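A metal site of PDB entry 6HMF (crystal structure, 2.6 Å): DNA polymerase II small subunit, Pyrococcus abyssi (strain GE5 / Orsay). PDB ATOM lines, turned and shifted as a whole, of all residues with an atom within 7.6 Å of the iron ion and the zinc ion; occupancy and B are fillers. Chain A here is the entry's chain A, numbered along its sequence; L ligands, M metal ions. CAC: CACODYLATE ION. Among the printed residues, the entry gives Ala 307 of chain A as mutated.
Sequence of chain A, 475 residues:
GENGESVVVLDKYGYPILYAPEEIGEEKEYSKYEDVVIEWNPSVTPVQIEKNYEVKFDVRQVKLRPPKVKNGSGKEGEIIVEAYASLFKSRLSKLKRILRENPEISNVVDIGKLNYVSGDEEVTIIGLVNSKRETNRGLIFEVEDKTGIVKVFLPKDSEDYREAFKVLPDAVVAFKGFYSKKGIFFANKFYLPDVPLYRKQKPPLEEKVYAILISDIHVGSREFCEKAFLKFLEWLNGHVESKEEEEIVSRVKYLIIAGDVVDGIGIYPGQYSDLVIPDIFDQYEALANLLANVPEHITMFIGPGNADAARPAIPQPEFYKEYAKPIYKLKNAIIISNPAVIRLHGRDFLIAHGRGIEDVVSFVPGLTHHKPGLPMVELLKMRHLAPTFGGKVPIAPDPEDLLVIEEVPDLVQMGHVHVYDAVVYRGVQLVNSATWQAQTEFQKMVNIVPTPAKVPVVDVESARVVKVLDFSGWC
A ring nitrogen (NE2) of His 416 sits at hydrogen-bond distance from the side-chain carboxylate of Glu 358 (3.0 Å). The side-chain carboxylate (OD1) of Asp 260 sits at hydrogen-bond distance from the backbone NH (N) of Ala 307, at 2.8 Å. The side-chain hydroxyl (OG1) of Thr 435 lies within hydrogen-bond range of the backbone carbonyl oxygen (O) of Asp 216, 2.7 Å away. The backbone carbonyl oxygen of His 353 lies within hydrogen-bond range of the backbone NH of Gly 415, at 2.8 Å. The backbone carbonyl oxygen (O) of Ala 258 sits at hydrogen-bond distance from a ring nitrogen (ND1) of His 353, 2.8 Å away. N of Ile 217 is in hydrogen-bond range of O of Asp 260, at 3.0 Å. The backbone NH of Asp 260 lies within hydrogen-bond range of the side-chain carboxylate of Asp 308 (2.9 Å). The backbone NH (N) of Asp 216 sits at hydrogen-bond distance from the backbone carbonyl oxygen (O) of Gly 259, 2.8 Å away.
The nearest printed residue that does not touch the zinc ion is Arg 355 (4.9 Å).
An oxygen (O2) of the ligand binds the iron ion, at 1.8 Å. OD2 of Asp 216 is bound to the iron ion (2.0 Å). The iron ion is bound by a ring nitrogen (NE2) of His 218 (2.2 Å). NE2 of His 418 binds the iron ion (2.3 Å). OD2 of Asp 260 is bound to the iron ion, 2.5 Å away.
The zinc ion is bound by the side-chain carboxylate of Asp 260, the side-chain amide oxygen of Asn 306, a ring nitrogen (NE2) of His 353 and a ring nitrogen (ND1) of His 416. Slightly farther from the zinc ion lies O2 of the ligand (2.8 Å).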
ATOM      1  N   SER A 215     -22.408   5.461 -20.903  1.00  0.00           N
ATOM      2  CA  SER A 215     -23.433   6.292 -20.276  1.00  0.00           C
ATOM      3  C   SER A 215     -24.783   5.925 -20.890  1.00  0.00           C
ATOM      4  O   SER A 215     -24.831   5.138 -21.841  1.00  0.00           O
ATOM      5  CB  SER A 215     -23.158   7.784 -20.469  1.00  0.00           C
ATOM      6  OG  SER A 215     -23.303   8.199 -21.817  1.00  0.00           O
ATOM      7  N   ASP A 216     -25.844   6.517 -20.333  1.00  0.00           N
ATOM      8  CA  ASP A 216     -27.235   6.416 -20.763  1.00  0.00           C
ATOM      9  C   ASP A 216     -27.625   4.979 -21.116  1.00  0.00           C
ATOM     10  O   ASP A 216     -28.046   4.685 -22.237  1.00  0.00           O
ATOM     11  CB  ASP A 216     -27.505   7.408 -21.892  1.00  0.00           C
ATOM     12  CG  ASP A 216     -27.263   8.843 -21.474  1.00  0.00           C
ATOM     13  OD1 ASP A 216     -26.085   9.254 -21.447  1.00  0.00           O
ATOM     14  OD2 ASP A 216     -28.241   9.526 -21.143  1.00  0.00           O
ATOM     15  N   ILE A 217     -27.454   4.084 -20.137  1.00  0.00           N
ATOM     16  CA  ILE A 217     -27.792   2.669 -20.265  1.00  0.00           C
ATOM     17  C   ILE A 217     -29.321   2.528 -20.366  1.00  0.00           C
ATOM     18  O   ILE A 217     -29.805   1.798 -21.224  1.00  0.00           O
ATOM     19  CB  ILE A 217     -27.164   1.825 -19.126  1.00  0.00           C
ATOM     20  CG1 ILE A 217     -25.647   2.146 -18.945  1.00  0.00           C
ATOM     21  CG2 ILE A 217     -27.392   0.327 -19.400  1.00  0.00           C
ATOM     22  CD1 ILE A 217     -24.963   1.487 -17.751  1.00  0.00           C
ATOM     23  N   HIS A 218     -30.055   3.305 -19.537  1.00  0.00           N
ATOM     24  CA  HIS A 218     -31.517   3.364 -19.499  1.00  0.00           C
ATOM     25  C   HIS A 218     -32.173   2.015 -19.246  1.00  0.00           C
ATOM     26  O   HIS A 218     -33.152   1.670 -19.925  1.00  0.00           O
ATOM     27  CB  HIS A 218     -32.111   4.061 -20.732  1.00  0.00           C
ATOM     28  CG  HIS A 218     -31.879   5.533 -20.742  1.00  0.00           C
ATOM     29  ND1 HIS A 218     -32.766   6.411 -20.155  1.00  0.00           N
ATOM     30  CD2 HIS A 218     -30.825   6.232 -21.213  1.00  0.00           C
ATOM     31  CE1 HIS A 218     -32.244   7.616 -20.301  1.00  0.00           C
ATOM     32  NE2 HIS A 218     -31.077   7.555 -20.925  1.00  0.00           N
ATOM     33  N   ALA A 258     -21.315   7.724 -17.072  1.00  0.00           N
ATOM     34  CA  ALA A 258     -21.746   9.122 -16.954  1.00  0.00           C
ATOM     35  C   ALA A 258     -23.268   9.375 -17.013  1.00  0.00           C
ATOM     36  O   ALA A 258     -23.735  10.160 -17.835  1.00  0.00           O
ATOM     37  CB  ALA A 258     -21.028   9.977 -17.988  1.00  0.00           C
ATOM     38  N   GLY A 259     -23.999   8.759 -16.097  1.00  0.00           N
ATOM     39  CA  GLY A 259     -25.428   9.012 -15.922  1.00  0.00           C
ATOM     40  C   GLY A 259     -26.437   8.251 -16.744  1.00  0.00           C
ATOM     41  O   GLY A 259     -26.093   7.578 -17.717  1.00  0.00           O
ATOM     42  N   ASP A 260     -27.716   8.407 -16.343  1.00  0.00           N
ATOM     43  CA  ASP A 260     -28.916   7.766 -16.871  1.00  0.00           C
ATOM     44  C   ASP A 260     -28.726   6.249 -16.979  1.00  0.00           C
ATOM     45  O   ASP A 260     -28.983   5.628 -18.021  1.00  0.00           O
ATOM     46  CB  ASP A 260     -29.397   8.415 -18.164  1.00  0.00           C
ATOM     47  CG  ASP A 260     -29.970   9.811 -17.989  1.00  0.00           C
ATOM     48  OD1 ASP A 260     -30.291  10.188 -16.846  1.00  0.00           O
ATOM     49  OD2 ASP A 260     -30.083  10.532 -18.988  1.00  0.00           O
ATOM     50  N   VAL A 261     -28.265   5.659 -15.873  1.00  0.00           N
ATOM     51  CA  VAL A 261     -27.957   4.238 -15.728  1.00  0.00           C
ATOM     52  C   VAL A 261     -29.262   3.427 -15.733  1.00  0.00           C
ATOM     53  O   VAL A 261     -29.276   2.295 -16.209  1.00  0.00           O
ATOM     54  CB  VAL A 261     -26.994   3.955 -14.524  1.00  0.00           C
ATOM     55  CG1 VAL A 261     -25.691   4.730 -14.679  1.00  0.00           C
ATOM     56  CG2 VAL A 261     -27.633   4.284 -13.174  1.00  0.00           C
ATOM     57  N   VAL A 262     -30.367   4.047 -15.276  1.00  0.00           N
ATOM     58  CA  VAL A 262     -31.721   3.482 -15.313  1.00  0.00           C
ATOM     59  C   VAL A 262     -32.631   4.467 -16.093  1.00  0.00           C
ATOM     60  O   VAL A 262     -32.282   5.644 -16.214  1.00  0.00           O
ATOM     61  CB  VAL A 262     -32.296   3.099 -13.908  1.00  0.00           C
ATOM     62  CG1 VAL A 262     -31.415   2.092 -13.185  1.00  0.00           C
ATOM     63  CG2 VAL A 262     -32.575   4.324 -13.048  1.00  0.00           C
ATOM     64  N   ASP A 263     -33.790   4.005 -16.614  1.00  0.00           N
ATOM     65  CA  ASP A 263     -34.700   4.898 -17.343  1.00  0.00           C
ATOM     66  C   ASP A 263     -35.511   5.798 -16.399  1.00  0.00           C
ATOM     67  O   ASP A 263     -35.974   6.858 -16.815  1.00  0.00           O
ATOM     68  CB  ASP A 263     -35.613   4.148 -18.345  1.00  0.00           C
ATOM     69  CG  ASP A 263     -36.233   5.049 -19.399  1.00  0.00           C
ATOM     70  OD1 ASP A 263     -35.475   5.754 -20.093  1.00  0.00           O
ATOM     71  OD2 ASP A 263     -37.483   5.039 -19.532  1.00  0.00           O
ATOM     72  N   ILE A 267     -40.309  10.564 -15.526  1.00  0.00           N
ATOM     73  CA  ILE A 267     -39.351  11.518 -16.115  1.00  0.00           C
ATOM     74  C   ILE A 267     -40.062  12.445 -17.127  1.00  0.00           C
ATOM     75  O   ILE A 267     -39.790  13.650 -17.171  1.00  0.00           O
ATOM     76  CB  ILE A 267     -38.092  10.803 -16.683  1.00  0.00           C
ATOM     77  CG1 ILE A 267     -37.377   9.925 -15.612  1.00  0.00           C
ATOM     78  CG2 ILE A 267     -37.092  11.777 -17.344  1.00  0.00           C
ATOM     79  CD1 ILE A 267     -36.987  10.606 -14.264  1.00  0.00           C
ATOM     80  N   GLY A 305     -27.473  10.686 -13.545  1.00  0.00           N
ATOM     81  CA  GLY A 305     -28.014  11.500 -14.627  1.00  0.00           C
ATOM     82  C   GLY A 305     -29.371  12.043 -14.223  1.00  0.00           C
ATOM     83  O   GLY A 305     -29.756  11.895 -13.058  1.00  0.00           O
ATOM     84  N   ASN A 306     -30.129  12.646 -15.151  1.00  0.00           N
ATOM     85  CA  ASN A 306     -31.442  13.227 -14.833  1.00  0.00           C
ATOM     86  C   ASN A 306     -32.590  12.197 -14.716  1.00  0.00           C
ATOM     87  O   ASN A 306     -33.643  12.524 -14.168  1.00  0.00           O
ATOM     88  CB  ASN A 306     -31.813  14.360 -15.805  1.00  0.00           C
ATOM     89  CG  ASN A 306     -31.816  13.940 -17.250  1.00  0.00           C
ATOM     90  OD1 ASN A 306     -30.785  13.580 -17.822  1.00  0.00           O
ATOM     91  ND2 ASN A 306     -32.995  13.986 -17.866  1.00  0.00           N
ATOM     92  N   ALA A 307     -32.397  10.949 -15.222  1.00  0.00           N
ATOM     93  CA  ALA A 307     -33.398   9.864 -15.176  1.00  0.00           C
ATOM     94  C   ALA A 307     -33.248   9.081 -13.901  1.00  0.00           C
ATOM     95  O   ALA A 307     -34.181   8.404 -13.468  1.00  0.00           O
ATOM     96  CB  ALA A 307     -33.248   8.938 -16.387  1.00  0.00           C
ATOM     97  N   ASP A 308     -32.069   9.170 -13.289  1.00  0.00           N
ATOM     98  CA  ASP A 308     -31.678   8.461 -12.070  1.00  0.00           C
ATOM     99  C   ASP A 308     -32.373   8.914 -10.803  1.00  0.00           C
ATOM    100  O   ASP A 308     -32.923  10.020 -10.735  1.00  0.00           O
ATOM    101  CB  ASP A 308     -30.154   8.539 -11.890  1.00  0.00           C
ATOM    102  CG  ASP A 308     -29.433   7.624 -12.861  1.00  0.00           C
ATOM    103  OD1 ASP A 308     -29.795   6.441 -12.938  1.00  0.00           O
ATOM    104  OD2 ASP A 308     -28.533   8.103 -13.556  1.00  0.00           O
ATOM    105  N   HIS A 353     -22.889  14.587 -16.582  1.00  0.00           N
ATOM    106  CA  HIS A 353     -23.936  13.937 -17.359  1.00  0.00           C
ATOM    107  C   HIS A 353     -24.147  14.578 -18.723  1.00  0.00           C
ATOM    108  O   HIS A 353     -24.348  13.860 -19.698  1.00  0.00           O
ATOM    109  CB  HIS A 353     -25.255  13.817 -16.598  1.00  0.00           C
ATOM    110  CG  HIS A 353     -26.279  13.040 -17.354  1.00  0.00           C
ATOM    111  ND1 HIS A 353     -26.007  11.769 -17.848  1.00  0.00           N
ATOM    112  CD2 HIS A 353     -27.516  13.401 -17.754  1.00  0.00           C
ATOM    113  CE1 HIS A 353     -27.089  11.412 -18.501  1.00  0.00           C
ATOM    114  NE2 HIS A 353     -28.028  12.358 -18.466  1.00  0.00           N
ATOM    115  N   GLY A 354     -24.087  15.900 -18.805  1.00  0.00           N
ATOM    116  CA  GLY A 354     -24.196  16.581 -20.098  1.00  0.00           C
ATOM    117  C   GLY A 354     -25.387  17.474 -20.296  1.00  0.00           C
ATOM    118  O   GLY A 354     -25.700  17.782 -21.454  1.00  0.00           O
ATOM    119  N   ARG A 355     -26.024  17.922 -19.199  1.00  0.00           N
ATOM    120  CA  ARG A 355     -27.186  18.813 -19.236  1.00  0.00           C
ATOM    121  C   ARG A 355     -26.891  20.131 -19.946  1.00  0.00           C
ATOM    122  O   ARG A 355     -27.774  20.678 -20.608  1.00  0.00           O
ATOM    123  CB  ARG A 355     -27.760  19.067 -17.827  1.00  0.00           C
ATOM    124  CG  ARG A 355     -28.325  17.840 -17.094  1.00  0.00           C
ATOM    125  CD  ARG A 355     -29.430  17.055 -17.821  1.00  0.00           C
ATOM    126  NE  ARG A 355     -30.535  17.906 -18.301  1.00  0.00           N
ATOM    127  CZ  ARG A 355     -31.610  18.246 -17.582  1.00  0.00           C
ATOM    128  NH1 ARG A 355     -31.732  17.817 -16.320  1.00  0.00           N
ATOM    129  NH2 ARG A 355     -32.544  19.025 -18.100  1.00  0.00           N
ATOM    130  N   GLU A 358     -27.476  20.698 -23.924  1.00  0.00           N
ATOM    131  CA  GLU A 358     -28.808  21.168 -24.285  1.00  0.00           C
ATOM    132  C   GLU A 358     -28.888  22.683 -24.296  1.00  0.00           C
ATOM    133  O   GLU A 358     -29.485  23.234 -25.222  1.00  0.00           O
ATOM    134  CB  GLU A 358     -29.859  20.634 -23.305  1.00  0.00           C
ATOM    135  CG  GLU A 358     -30.490  19.333 -23.758  1.00  0.00           C
ATOM    136  CD  GLU A 358     -31.713  18.931 -22.975  1.00  0.00           C
ATOM    137  OE1 GLU A 358     -31.680  18.965 -21.721  1.00  0.00           O
ATOM    138  OE2 GLU A 358     -32.691  18.509 -23.630  1.00  0.00           O
ATOM    139  N   GLY A 415     -22.585  12.457 -21.293  1.00  0.00           N
ATOM    140  CA  GLY A 415     -23.607  11.597 -21.858  1.00  0.00           C
ATOM    141  C   GLY A 415     -24.780  12.469 -22.254  1.00  0.00           C
ATOM    142  O   GLY A 415     -24.610  13.483 -22.942  1.00  0.00           O
ATOM    143  N   HIS A 416     -25.976  12.114 -21.773  1.00  0.00           N
ATOM    144  CA  HIS A 416     -27.246  12.830 -21.905  1.00  0.00           C
ATOM    145  C   HIS A 416     -27.825  12.948 -23.326  1.00  0.00           C
ATOM    146  O   HIS A 416     -28.991  12.626 -23.495  1.00  0.00           O
ATOM    147  CB  HIS A 416     -27.158  14.230 -21.246  1.00  0.00           C
ATOM    148  CG  HIS A 416     -28.450  14.981 -21.237  1.00  0.00           C
ATOM    149  ND1 HIS A 416     -29.574  14.475 -20.592  1.00  0.00           N
ATOM    150  CD2 HIS A 416     -28.766  16.160 -21.784  1.00  0.00           C
ATOM    151  CE1 HIS A 416     -30.539  15.358 -20.795  1.00  0.00           C
ATOM    152  NE2 HIS A 416     -30.093  16.389 -21.503  1.00  0.00           N
ATOM    153  N   VAL A 417     -27.068  13.427 -24.331  1.00  0.00           N
ATOM    154  CA  VAL A 417     -27.622  13.654 -25.685  1.00  0.00           C
ATOM    155  C   VAL A 417     -27.814  12.379 -26.540  1.00  0.00           C
ATOM    156  O   VAL A 417     -28.488  12.453 -27.599  1.00  0.00           O
ATOM    157  CB  VAL A 417     -26.882  14.749 -26.483  1.00  0.00           C
ATOM    158  CG1 VAL A 417     -26.870  16.057 -25.718  1.00  0.00           C
ATOM    159  CG2 VAL A 417     -25.471  14.305 -26.872  1.00  0.00           C
ATOM    160  N   HIS A 418     -27.223  11.236 -26.132  1.00  0.00           N
ATOM    161  CA  HIS A 418     -27.373   9.921 -26.786  1.00  0.00           C
ATOM    162  C   HIS A 418     -26.703   9.804 -28.154  1.00  0.00           C
ATOM    163  O   HIS A 418     -26.985   8.854 -28.882  1.00  0.00           O
ATOM    164  CB  HIS A 418     -28.867   9.532 -26.889  1.00  0.00           C
ATOM    165  CG  HIS A 418     -29.503   9.206 -25.575  1.00  0.00           C
ATOM    166  ND1 HIS A 418     -30.661   8.478 -25.506  1.00  0.00           N
ATOM    167  CD2 HIS A 418     -29.102   9.518 -24.308  1.00  0.00           C
ATOM    168  CE1 HIS A 418     -30.951   8.370 -24.225  1.00  0.00           C
ATOM    169  NE2 HIS A 418     -30.040   8.977 -23.468  1.00  0.00           N
ATOM    170  N   ALA A 434     -22.333   8.353 -25.765  1.00  0.00           N
ATOM    171  CA  ALA A 434     -23.588   7.954 -26.405  1.00  0.00           C
ATOM    172  C   ALA A 434     -24.631   7.341 -25.447  1.00  0.00           C
ATOM    173  O   ALA A 434     -24.961   7.966 -24.432  1.00  0.00           O
ATOM    174  CB  ALA A 434     -23.325   7.025 -27.593  1.00  0.00           C
ATOM    175  N   THR A 435     -25.200   6.161 -25.818  1.00  0.00           N
ATOM    176  CA  THR A 435     -26.286   5.493 -25.099  1.00  0.00           C
ATOM    177  C   THR A 435     -26.388   4.004 -25.429  1.00  0.00           C
ATOM    178  O   THR A 435     -25.825   3.537 -26.428  1.00  0.00           O
ATOM    179  CB  THR A 435     -27.633   6.188 -25.475  1.00  0.00           C
ATOM    180  OG1 THR A 435     -28.691   5.701 -24.659  1.00  0.00           O
ATOM    181  CG2 THR A 435     -28.004   6.041 -26.969  1.00  0.00           C
ATOM    182  N   GLN A 437     -29.635   2.914 -25.399  1.00  0.00           N
ATOM    183  CA  GLN A 437     -31.055   3.040 -25.642  1.00  0.00           C
ATOM    184  C   GLN A 437     -31.338   3.444 -27.080  1.00  0.00           C
ATOM    185  O   GLN A 437     -30.867   4.492 -27.520  1.00  0.00           O
ATOM    186  CB  GLN A 437     -31.687   4.047 -24.667  1.00  0.00           C
ATOM    187  CG  GLN A 437     -33.188   4.260 -24.881  1.00  0.00           C
ATOM    188  CD  GLN A 437     -33.812   5.257 -23.948  1.00  0.00           C
ATOM    189  OE1 GLN A 437     -33.447   6.445 -23.895  1.00  0.00           O
ATOM    190  NE2 GLN A 437     -34.834   4.819 -23.249  1.00  0.00           N
ATOM    191  N   GLN A 443     -38.432  10.433 -28.219  1.00  0.00           N
ATOM    192  CA  GLN A 443     -37.233  10.907 -28.916  1.00  0.00           C
ATOM    193  C   GLN A 443     -37.562  11.229 -30.390  1.00  0.00           C
ATOM    194  O   GLN A 443     -37.167  12.277 -30.887  1.00  0.00           O
ATOM    195  CB  GLN A 443     -36.083   9.899 -28.797  1.00  0.00           C
ATOM    196  CG  GLN A 443     -35.419   9.893 -27.414  1.00  0.00           C
ATOM    197  CD  GLN A 443     -34.608   8.647 -27.078  1.00  0.00           C
ATOM    198  OE1 GLN A 443     -34.414   7.756 -27.895  1.00  0.00           O
ATOM    199  NE2 GLN A 443     -34.104   8.580 -25.871  1.00  0.00           N
HETATM  200 AS   CAC L   1     -32.645  11.643 -21.531  1.00  0.00          AS
HETATM  201  O1  CAC L   1     -33.194  12.497 -20.221  1.00  0.00           O
HETATM  202  O2  CAC L   1     -31.146  10.922 -21.578  1.00  0.00           O
HETATM  203  C1  CAC L   1     -34.013  10.310 -22.031  1.00  0.00           C
HETATM  204  C2  CAC L   1     -32.792  12.774 -23.153  1.00  0.00           C
HETATM  205 FE    FE M   1     -30.191   9.494 -21.235  1.00  0.00          FE
HETATM  206 ZN    ZN M   2     -30.006  12.513 -19.523  1.00  0.00          ZN
